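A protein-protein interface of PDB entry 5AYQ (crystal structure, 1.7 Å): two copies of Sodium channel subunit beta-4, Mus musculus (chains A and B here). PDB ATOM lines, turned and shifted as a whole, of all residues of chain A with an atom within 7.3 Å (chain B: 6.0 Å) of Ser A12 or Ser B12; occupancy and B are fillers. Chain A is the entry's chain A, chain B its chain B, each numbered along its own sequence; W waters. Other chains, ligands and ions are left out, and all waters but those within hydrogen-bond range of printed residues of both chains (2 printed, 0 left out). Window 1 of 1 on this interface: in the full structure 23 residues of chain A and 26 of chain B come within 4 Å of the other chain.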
ATOM      1  N   GLU A  10     -30.248  -3.448  23.034  1.00  0.00           N
ATOM      2  CA  GLU A  10     -29.292  -2.448  22.569  1.00  0.00           C
ATOM      3  C   GLU A  10     -28.265  -2.118  23.652  1.00  0.00           C
ATOM      4  O   GLU A  10     -28.536  -2.278  24.842  1.00  0.00           O
ATOM      5  CB  GLU A  10     -30.027  -1.181  22.126  1.00  0.00           C
ATOM      6  CG  GLU A  10     -29.167  -0.194  21.343  1.00  0.00           C
ATOM      7  CD  GLU A  10     -28.507  -0.819  20.127  1.00  0.00           C
ATOM      8  OE1 GLU A  10     -29.228  -1.146  19.159  1.00  0.00           O
ATOM      9  OE2 GLU A  10     -27.267  -0.989  20.141  1.00  0.00           O
ATOM     10  N   VAL A  11     -27.083  -1.676  23.229  1.00  0.00           N
ATOM     11  CA  VAL A  11     -26.052  -1.210  24.152  1.00  0.00           C
ATOM     12  C   VAL A  11     -25.561   0.177  23.781  1.00  0.00           C
ATOM     13  O   VAL A  11     -25.653   0.599  22.629  1.00  0.00           O
ATOM     14  CB  VAL A  11     -24.830  -2.150  24.193  1.00  0.00           C
ATOM     15  CG1 VAL A  11     -25.155  -3.402  24.950  1.00  0.00           C
ATOM     16  CG2 VAL A  11     -24.346  -2.473  22.777  1.00  0.00           C
ATOM     17  N   SER A  12     -25.020   0.873  24.772  1.00  0.00           N
ATOM     18  CA  SER A  12     -24.523   2.225  24.588  1.00  0.00           C
ATOM     19  C   SER A  12     -23.306   2.458  25.467  1.00  0.00           C
ATOM     20  O   SER A  12     -23.200   1.874  26.547  1.00  0.00           O
ATOM     21  CB  SER A  12     -25.614   3.243  24.920  1.00  0.00           C
ATOM     22  OG  SER A  12     -25.114   4.561  24.855  1.00  0.00           O
ATOM     23  N   VAL A  13     -22.391   3.309  25.014  1.00  0.00           N
ATOM     24  CA  VAL A  13     -21.277   3.706  25.859  1.00  0.00           C
ATOM     25  C   VAL A  13     -21.644   4.945  26.668  1.00  0.00           C
ATOM     26  O   VAL A  13     -20.811   5.478  27.400  1.00  0.00           O
ATOM     27  CB  VAL A  13     -19.990   3.971  25.049  1.00  0.00           C
ATOM     28  CG1 VAL A  13     -19.541   2.705  24.335  1.00  0.00           C
ATOM     29  CG2 VAL A  13     -20.192   5.109  24.063  1.00  0.00           C
ATOM     30  N   GLY A  14     -22.890   5.400  26.535  1.00  0.00           N
ATOM     31  CA  GLY A  14     -23.405   6.458  27.387  1.00  0.00           C
ATOM     32  C   GLY A  14     -24.074   7.609  26.658  1.00  0.00           C
ATOM     33  O   GLY A  14     -24.180   7.603  25.430  1.00  0.00           O
ATOM     34  N   LYS A  15     -24.525   8.598  27.427  1.00  0.00           N
ATOM     35  CA  LYS A  15     -25.164   9.781  26.857  1.00  0.00           C
ATOM     36  C   LYS A  15     -24.145  10.896  26.661  1.00  0.00           C
ATOM     37  O   LYS A  15     -24.485  11.992  26.225  1.00  0.00           O
ATOM     38  CB  LYS A  15     -26.310  10.254  27.752  1.00  0.00           C
ATOM     39  CG  LYS A  15     -27.519   9.334  27.732  1.00  0.00           C
ATOM     40  CD  LYS A  15     -28.513   9.682  28.831  1.00  0.00           C
ATOM     41  CE  LYS A  15     -29.050  11.095  28.673  1.00  0.00           C
ATOM     42  NZ  LYS A  15     -30.078  11.422  29.708  1.00  0.00           N
ATOM     43  N   ALA A  16     -22.890  10.612  26.980  1.00  0.00           N
ATOM     44  CA  ALA A  16     -21.846  11.613  26.844  1.00  0.00           C
ATOM     45  C   ALA A  16     -20.482  10.977  26.649  1.00  0.00           C
ATOM     46  O   ALA A  16     -20.236   9.843  27.085  1.00  0.00           O
ATOM     47  CB  ALA A  16     -21.831  12.535  28.057  1.00  0.00           C
ATOM     48  N   PRO A  30     -20.947  12.162  17.277  1.00  0.00           N
ATOM     49  CA  PRO A  30     -21.888  11.047  17.188  1.00  0.00           C
ATOM     50  C   PRO A  30     -23.131  11.203  18.042  1.00  0.00           C
ATOM     51  O   PRO A  30     -23.043  11.583  19.212  1.00  0.00           O
ATOM     52  CB  PRO A  30     -21.055   9.864  17.688  1.00  0.00           C
ATOM     53  CG  PRO A  30     -20.153  10.482  18.707  1.00  0.00           C
ATOM     54  CD  PRO A  30     -19.803  11.850  18.152  1.00  0.00           C
ATOM     55  N   CYS A  31     -24.281  10.868  17.466  1.00  0.00           N
ATOM     56  CA  CYS A  31     -25.508  10.762  18.240  1.00  0.00           C
ATOM     57  C   CYS A  31     -26.526   9.879  17.540  1.00  0.00           C
ATOM     58  O   CYS A  31     -26.778  10.031  16.345  1.00  0.00           O
ATOM     59  CB  CYS A  31     -26.123  12.147  18.493  1.00  0.00           C
ATOM     60  SG  CYS A  31     -27.606  12.078  19.526  1.00  0.00           S
ATOM     61  N   THR A  32     -27.103   8.953  18.301  1.00  0.00           N
ATOM     62  CA  THR A  32     -28.180   8.099  17.822  1.00  0.00           C
ATOM     63  C   THR A  32     -29.316   8.111  18.828  1.00  0.00           C
ATOM     64  O   THR A  32     -29.112   8.444  19.991  1.00  0.00           O
ATOM     65  CB  THR A  32     -27.714   6.643  17.614  1.00  0.00           C
ATOM     66  OG1 THR A  32     -27.348   6.085  18.883  1.00  0.00           O
ATOM     67  CG2 THR A  32     -26.525   6.586  16.677  1.00  0.00           C
ATOM     68  N   PHE A  33     -30.517   7.746  18.394  1.00  0.00           N
ATOM     69  CA  PHE A  33     -31.634   7.689  19.322  1.00  0.00           C
ATOM     70  C   PHE A  33     -32.520   6.497  19.010  1.00  0.00           C
ATOM     71  O   PHE A  33     -32.447   5.922  17.924  1.00  0.00           O
ATOM     72  CB  PHE A  33     -32.454   8.983  19.286  1.00  0.00           C
ATOM     73  CG  PHE A  33     -33.249   9.172  18.021  1.00  0.00           C
ATOM     74  CD1 PHE A  33     -34.538   8.664  17.909  1.00  0.00           C
ATOM     75  CD2 PHE A  33     -32.718   9.876  16.953  1.00  0.00           C
ATOM     76  CE1 PHE A  33     -35.267   8.830  16.746  1.00  0.00           C
ATOM     77  CE2 PHE A  33     -33.450  10.054  15.788  1.00  0.00           C
ATOM     78  CZ  PHE A  33     -34.727   9.530  15.687  1.00  0.00           C
ATOM     79  N   SER A  34     -33.357   6.128  19.971  1.00  0.00           N
ATOM     80  CA  SER A  34     -34.315   5.060  19.739  1.00  0.00           C
ATOM     81  C   SER A  34     -35.581   5.264  20.551  1.00  0.00           C
ATOM     82  O   SER A  34     -35.596   5.997  21.553  1.00  0.00           O
ATOM     83  CB  SER A  34     -33.696   3.698  20.054  1.00  0.00           C
ATOM     84  OG  SER A  34     -33.156   3.672  21.362  1.00  0.00           O
ATOM     85  N   ASN A  90     -31.226   4.900  14.643  1.00  0.00           N
ATOM     86  CA  ASN A  90     -31.571   6.208  14.131  1.00  0.00           C
ATOM     87  C   ASN A  90     -30.390   7.136  14.382  1.00  0.00           C
ATOM     88  O   ASN A  90     -30.187   7.601  15.503  1.00  0.00           O
ATOM     89  CB  ASN A  90     -32.846   6.733  14.789  1.00  0.00           C
ATOM     90  CG  ASN A  90     -34.023   5.786  14.611  1.00  0.00           C
ATOM     91  OD1 ASN A  90     -34.388   5.438  13.488  1.00  0.00           O
ATOM     92  ND2 ASN A  90     -34.615   5.356  15.719  1.00  0.00           N
ATOM     93  N   ILE A  92     -28.160  10.507  13.898  1.00  0.00           N
ATOM     94  CA  ILE A  92     -28.242  11.926  13.587  1.00  0.00           C
ATOM     95  C   ILE A  92     -26.910  12.622  13.855  1.00  0.00           C
ATOM     96  O   ILE A  92     -26.869  13.785  14.274  1.00  0.00           O
ATOM     97  CB  ILE A  92     -29.358  12.619  14.386  1.00  0.00           C
ATOM     98  CG1 ILE A  92     -29.293  12.217  15.860  1.00  0.00           C
ATOM     99  CG2 ILE A  92     -30.727  12.269  13.807  1.00  0.00           C
ATOM    100  CD1 ILE A  92     -30.324  12.931  16.724  1.00  0.00           C
ATOM    101  N   SER A  93     -25.824  11.897  13.607  1.00  0.00           N
ATOM    102  CA  SER A  93     -24.480  12.442  13.772  1.00  0.00           C
ATOM    103  C   SER A  93     -24.192  13.557  12.775  1.00  0.00           C
ATOM    104  O   SER A  93     -24.817  13.640  11.714  1.00  0.00           O
ATOM    105  CB  SER A  93     -23.434  11.340  13.616  1.00  0.00           C
ATOM    106  OG  SER A  93     -23.643  10.310  14.568  1.00  0.00           O
ATOM    107  N   CYS A 109     -26.657  17.363  21.600  1.00  0.00           N
ATOM    108  CA  CYS A 109     -27.658  16.927  20.646  1.00  0.00           C
ATOM    109  C   CYS A 109     -28.953  16.636  21.377  1.00  0.00           C
ATOM    110  O   CYS A 109     -29.028  15.729  22.208  1.00  0.00           O
ATOM    111  CB  CYS A 109     -27.194  15.703  19.864  1.00  0.00           C
ATOM    112  SG  CYS A 109     -28.366  15.252  18.572  1.00  0.00           S
ATOM    113  N   SER A 122     -31.090  14.335  25.698  1.00  0.00           N
ATOM    114  CA  SER A 122     -29.910  15.023  25.182  1.00  0.00           C
ATOM    115  C   SER A 122     -28.622  14.239  25.378  1.00  0.00           C
ATOM    116  O   SER A 122     -28.390  13.662  26.442  1.00  0.00           O
ATOM    117  CB  SER A 122     -29.763  16.394  25.849  1.00  0.00           C
ATOM    118  OG  SER A 122     -30.858  17.240  25.548  1.00  0.00           O
ATOM    119  N   ALA A 123     -27.782  14.229  24.349  1.00  0.00           N
ATOM    120  CA  ALA A 123     -26.433  13.694  24.479  1.00  0.00           C
ATOM    121  C   ALA A 123     -25.419  14.823  24.416  1.00  0.00           C
ATOM    122  O   ALA A 123     -25.700  15.907  23.902  1.00  0.00           O
ATOM    123  CB  ALA A 123     -26.145  12.666  23.406  1.00  0.00           C
ATOM    124  N   THR A 124     -24.232  14.554  24.937  1.00  0.00           N
ATOM    125  CA  THR A 124     -23.216  15.580  25.079  1.00  0.00           C
ATOM    126  C   THR A 124     -21.871  15.113  24.552  1.00  0.00           C
ATOM    127  O   THR A 124     -21.385  14.052  24.932  1.00  0.00           O
ATOM    128  CB  THR A 124     -23.050  15.989  26.556  1.00  0.00           C
ATOM    129  OG1 THR A 124     -24.280  16.533  27.049  1.00  0.00           O
ATOM    130  CG2 THR A 124     -21.948  17.011  26.699  1.00  0.00           C
ATOM    131  N   ILE A 125     -21.272  15.899  23.666  1.00  0.00           N
ATOM    132  CA  ILE A 125     -19.912  15.642  23.234  1.00  0.00           C
ATOM    133  C   ILE A 125     -19.027  16.769  23.733  1.00  0.00           C
ATOM    134  O   ILE A 125     -19.268  17.942  23.429  1.00  0.00           O
ATOM    135  CB  ILE A 125     -19.786  15.531  21.694  1.00  0.00           C
ATOM    136  CG1 ILE A 125     -20.750  14.477  21.136  1.00  0.00           C
ATOM    137  CG2 ILE A 125     -18.350  15.204  21.297  1.00  0.00           C
ATOM    138  CD1 ILE A 125     -20.554  13.090  21.722  1.00  0.00           C
ATOM    139  N   GLU B  10     -34.797   7.595  24.144  1.00  0.00           N
ATOM    140  CA  GLU B  10     -33.419   7.426  24.591  1.00  0.00           C
ATOM    141  C   GLU B  10     -32.430   8.034  23.597  1.00  0.00           C
ATOM    142  O   GLU B  10     -32.744   8.195  22.417  1.00  0.00           O
ATOM    143  CB  GLU B  10     -33.112   5.947  24.777  1.00  0.00           C
ATOM    144  CG  GLU B  10     -33.921   5.278  25.870  1.00  0.00           C
ATOM    145  CD  GLU B  10     -33.607   3.797  25.959  1.00  0.00           C
ATOM    146  OE1 GLU B  10     -32.762   3.329  25.163  1.00  0.00           O
ATOM    147  OE2 GLU B  10     -34.203   3.098  26.807  1.00  0.00           O
ATOM    148  N   VAL B  11     -31.237   8.370  24.075  1.00  0.00           N
ATOM    149  CA  VAL B  11     -30.192   8.930  23.224  1.00  0.00           C
ATOM    150  C   VAL B  11     -28.837   8.328  23.610  1.00  0.00           C
ATOM    151  O   VAL B  11     -28.589   8.039  24.781  1.00  0.00           O
ATOM    152  CB  VAL B  11     -30.142  10.476  23.330  1.00  0.00           C
ATOM    153  CG1 VAL B  11     -29.092  11.039  22.424  1.00  0.00           C
ATOM    154  CG2 VAL B  11     -31.480  11.089  22.974  1.00  0.00           C
ATOM    155  N   SER B  12     -27.965   8.146  22.622  1.00  0.00           N
ATOM    156  CA  SER B  12     -26.663   7.531  22.833  1.00  0.00           C
ATOM    157  C   SER B  12     -25.592   8.198  21.978  1.00  0.00           C
ATOM    158  O   SER B  12     -25.873   8.678  20.877  1.00  0.00           O
ATOM    159  CB  SER B  12     -26.733   6.035  22.507  1.00  0.00           C
ATOM    160  OG  SER B  12     -25.447   5.435  22.507  1.00  0.00           O
ATOM    161  N   VAL B  13     -24.360   8.215  22.474  1.00  0.00           N
ATOM    162  CA  VAL B  13     -23.241   8.672  21.660  1.00  0.00           C
ATOM    163  C   VAL B  13     -22.641   7.516  20.859  1.00  0.00           C
ATOM    164  O   VAL B  13     -21.652   7.695  20.151  1.00  0.00           O
ATOM    165  CB  VAL B  13     -22.137   9.333  22.509  1.00  0.00           C
ATOM    166  CG1 VAL B  13     -22.681  10.551  23.237  1.00  0.00           C
ATOM    167  CG2 VAL B  13     -21.534   8.330  23.493  1.00  0.00           C
ATOM    168  N   GLY B  14     -23.246   6.334  20.962  1.00  0.00           N
ATOM    169  CA  GLY B  14     -22.836   5.210  20.139  1.00  0.00           C
ATOM    170  C   GLY B  14     -22.545   3.928  20.896  1.00  0.00           C
ATOM    171  O   GLY B  14     -22.631   3.878  22.124  1.00  0.00           O
ATOM    172  N   LYS B  15     -22.208   2.887  20.142  1.00  0.00           N
ATOM    173  CA  LYS B  15     -21.850   1.595  20.718  1.00  0.00           C
ATOM    174  C   LYS B  15     -20.348   1.504  20.937  1.00  0.00           C
ATOM    175  O   LYS B  15     -19.841   0.482  21.388  1.00  0.00           O
ATOM    176  CB  LYS B  15     -22.318   0.455  19.808  1.00  0.00           C
ATOM    177  CG  LYS B  15     -23.825   0.357  19.672  1.00  0.00           C
ATOM    178  CD  LYS B  15     -24.220  -0.582  18.545  1.00  0.00           C
ATOM    179  CE  LYS B  15     -23.909  -2.024  18.893  1.00  0.00           C
ATOM    180  NZ  LYS B  15     -24.303  -2.968  17.806  1.00  0.00           N
ATOM    181  N   PRO B  30     -17.421   2.756  30.421  1.00  0.00           N
ATOM    182  CA  PRO B  30     -18.879   2.910  30.455  1.00  0.00           C
ATOM    183  C   PRO B  30     -19.639   1.962  29.550  1.00  0.00           C
ATOM    184  O   PRO B  30     -19.248   1.748  28.406  1.00  0.00           O
ATOM    185  CB  PRO B  30     -19.076   4.350  29.981  1.00  0.00           C
ATOM    186  CG  PRO B  30     -17.940   4.558  29.019  1.00  0.00           C
ATOM    187  CD  PRO B  30     -16.772   3.792  29.598  1.00  0.00           C
ATOM    188  N   CYS B  31     -20.739   1.420  30.062  1.00  0.00           N
ATOM    189  CA  CYS B  31     -21.670   0.672  29.238  1.00  0.00           C
ATOM    190  C   CYS B  31     -23.040   0.623  29.894  1.00  0.00           C
ATOM    191  O   CYS B  31     -23.161   0.358  31.095  1.00  0.00           O
ATOM    192  CB  CYS B  31     -21.171  -0.756  28.980  1.00  0.00           C
ATOM    193  SG  CYS B  31     -22.285  -1.701  27.902  1.00  0.00           S
ATOM    194  N   THR B  32     -24.065   0.888  29.093  1.00  0.00           N
ATOM    195  CA  THR B  32     -25.444   0.727  29.519  1.00  0.00           C
ATOM    196  C   THR B  32     -26.184  -0.095  28.482  1.00  0.00           C
ATOM    197  O   THR B  32     -25.736  -0.211  27.345  1.00  0.00           O
ATOM    198  CB  THR B  32     -26.155   2.084  29.705  1.00  0.00           C
ATOM    199  OG1 THR B  32     -26.262   2.747  28.438  1.00  0.00           O
ATOM    200  CG2 THR B  32     -25.380   2.967  30.669  1.00  0.00           C
ATOM    201  N   PHE B  33     -27.312  -0.679  28.861  1.00  0.00           N
ATOM    202  CA  PHE B  33     -28.086  -1.447  27.897  1.00  0.00           C
ATOM    203  C   PHE B  33     -29.565  -1.138  28.046  1.00  0.00           C
ATOM    204  O   PHE B  33     -30.012  -0.639  29.081  1.00  0.00           O
ATOM    205  CB  PHE B  33     -27.832  -2.955  28.046  1.00  0.00           C
ATOM    206  CG  PHE B  33     -28.357  -3.544  29.329  1.00  0.00           C
ATOM    207  CD1 PHE B  33     -29.656  -4.029  29.407  1.00  0.00           C
ATOM    208  CD2 PHE B  33     -27.548  -3.623  30.449  1.00  0.00           C
ATOM    209  CE1 PHE B  33     -30.139  -4.571  30.584  1.00  0.00           C
ATOM    210  CE2 PHE B  33     -28.023  -4.167  31.628  1.00  0.00           C
ATOM    211  CZ  PHE B  33     -29.322  -4.642  31.696  1.00  0.00           C
ATOM    212  N   ALA B 123     -20.770  -3.544  23.118  1.00  0.00           N
ATOM    213  CA  ALA B 123     -20.221  -2.204  23.016  1.00  0.00           C
ATOM    214  C   ALA B 123     -18.711  -2.278  23.150  1.00  0.00           C
ATOM    215  O   ALA B 123     -18.181  -3.232  23.716  1.00  0.00           O
ATOM    216  CB  ALA B 123     -20.816  -1.292  24.076  1.00  0.00           C
HETATM  217  O   HOH W   1     -25.939   2.983  21.242  1.00  0.00           O
HETATM  218  O   HOH W   2     -27.221   6.108  26.120  1.00  0.00           O
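The side-chain hydroxyl (OG) of Ser A12 lies within hydrogen-bond range of the side-chain hydroxyl (OG) of Ser B12 (2.5 Å).
The backbone carbonyl oxygen of Gly A14 is in hydrogen-bond range of the backbone NH of Val B13, 3.0 Å away.
O of Ser A12 lies within hydrogen-bond range of N of Thr B32, at 2.9 Å.
The backbone carbonyl oxygen of Ser B12 sits at hydrogen-bond distance from the backbone NH of Thr A32 (2.9 Å).
The backbone carbonyl oxygen (O) of Gly B14 sits at hydrogen-bond distance from the backbone NH (N) of Val A13 (3.0 Å).
The backbone carbonyl oxygen (O) of Ser A34 sits at hydrogen-bond distance from the backbone NH (N) of Glu B10 (3.1 Å).
The backbone carbonyl oxygen (O) of Ala A123 is in hydrogen-bond range of the backbone NH (N) of Cys A109 (2.9 Å).
SG of Cys A109 is in hydrogen-bond range of SG of Cys A31.
The backbone NH of Gly A14 sits at hydrogen-bond distance from the side-chain hydroxyl of Ser A12 (2.9 Å).
O of Cys A31 is in hydrogen-bond range of N of Ile A92 (2.9 Å).
O of Lys A15 is in hydrogen-bond range of N of Thr A124 (2.9 Å).
The backbone NH of Cys A31 lies within hydrogen-bond range of the side-chain hydroxyl of Ser A93 (3.0 Å).
Glu A10 touches Lys B15 (OE2 to CD, 3.5 Å).
CG of Lys B15 touches O of Val A11 (3.5 Å).
Val B13 touches Val A13 (CG2 to CG2, 3.5 Å).
Lys B15 touches Val A13.
Val A13 touches Pro B30.
C of Lys A15 touches CG1 of Val B13, at 3.7 Å.
Val B13 touches Ala A16 (CG1 to N, 3.7 Å).
Cys A31 touches Val B11.
O of Glu B10 touches CB of Phe A33 (3.2 Å).
Val B13 touches Ile A125 (CG1 to CD1, 3.6 Å).
Of the printed residues of chain B, Ser A12 touches Ser B12 (2.5 Å), Gly B14 (3.5 Å), Cys B31 (3.3 Å) and Thr B32 (2.9 Å).
Ser B12 touches just these residues of chain A: Ser A12, Gly A14, Cys A31 and Thr A32.
Printed residues of chain B within 4 Å of Thr A32: Val B11 (3.4 Å) and Ser B12 (2.9 Å).
Of the printed residues of chain B, Gly A14 touches Ser B12 (3.6 Å) and Val B13 (3.0 Å).
Printed residues of chain A within 4 Å of Pro B30: Val A13 (3.3 Å).
Asn A90 touches none of the printed residues of chain B.
Thr A124 touches none of the printed residues of chain B.
The nearest residue of chain B that does not touch Ser A12 is Pro B30 (4.4 Å).
The nearest residue of chain A that does not touch Ser B12 is Pro A30 (4.4 Å).
Of the 20 printed residues of chain A, 14 touch a printed residue of chain B.
Along chain A the printed residues that touch a printed residue of chain B span positions 10 to 125.
Of the 11 printed residues of chain B, 11 touch a printed residue of chain A.
Hydrophobic or aromatic side chains of chain B within 4 Å of the printed part of chain A: Val B11, Val B13, Pro B30, Phe B33 and Ala B123.
Val A11 touches Lys B15, and with the chains exchanged Lys A15 touches Val B11.
Ser A12 touches Thr B32, and with the chains exchanged Thr A32 touches Ser B12.
Val A13 touches Lys B15, and with the chains exchanged Lys A15 touches Val B13.
Cys A31 touches Val B11, but with the chains exchanged Val A11 does not touch Cys B31 (4.5 Å).
11 positions are printed for both chains.
Of the 27 pairs that touch across the chains among the printed residues, 22 have their exchanged pair printed and touching as well.
Water W2 lies within hydrogen-bond range of the backbone carbonyl oxygen (O) of Val B11, the side-chain hydroxyl (OG) of Ser A12 and the backbone carbonyl oxygen (O) of Gly A14.
Water W1 lies within hydrogen-bond range of the backbone carbonyl oxygen (O) of Val A11 and the side-chain hydroxyl (OG) of Ser B12.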
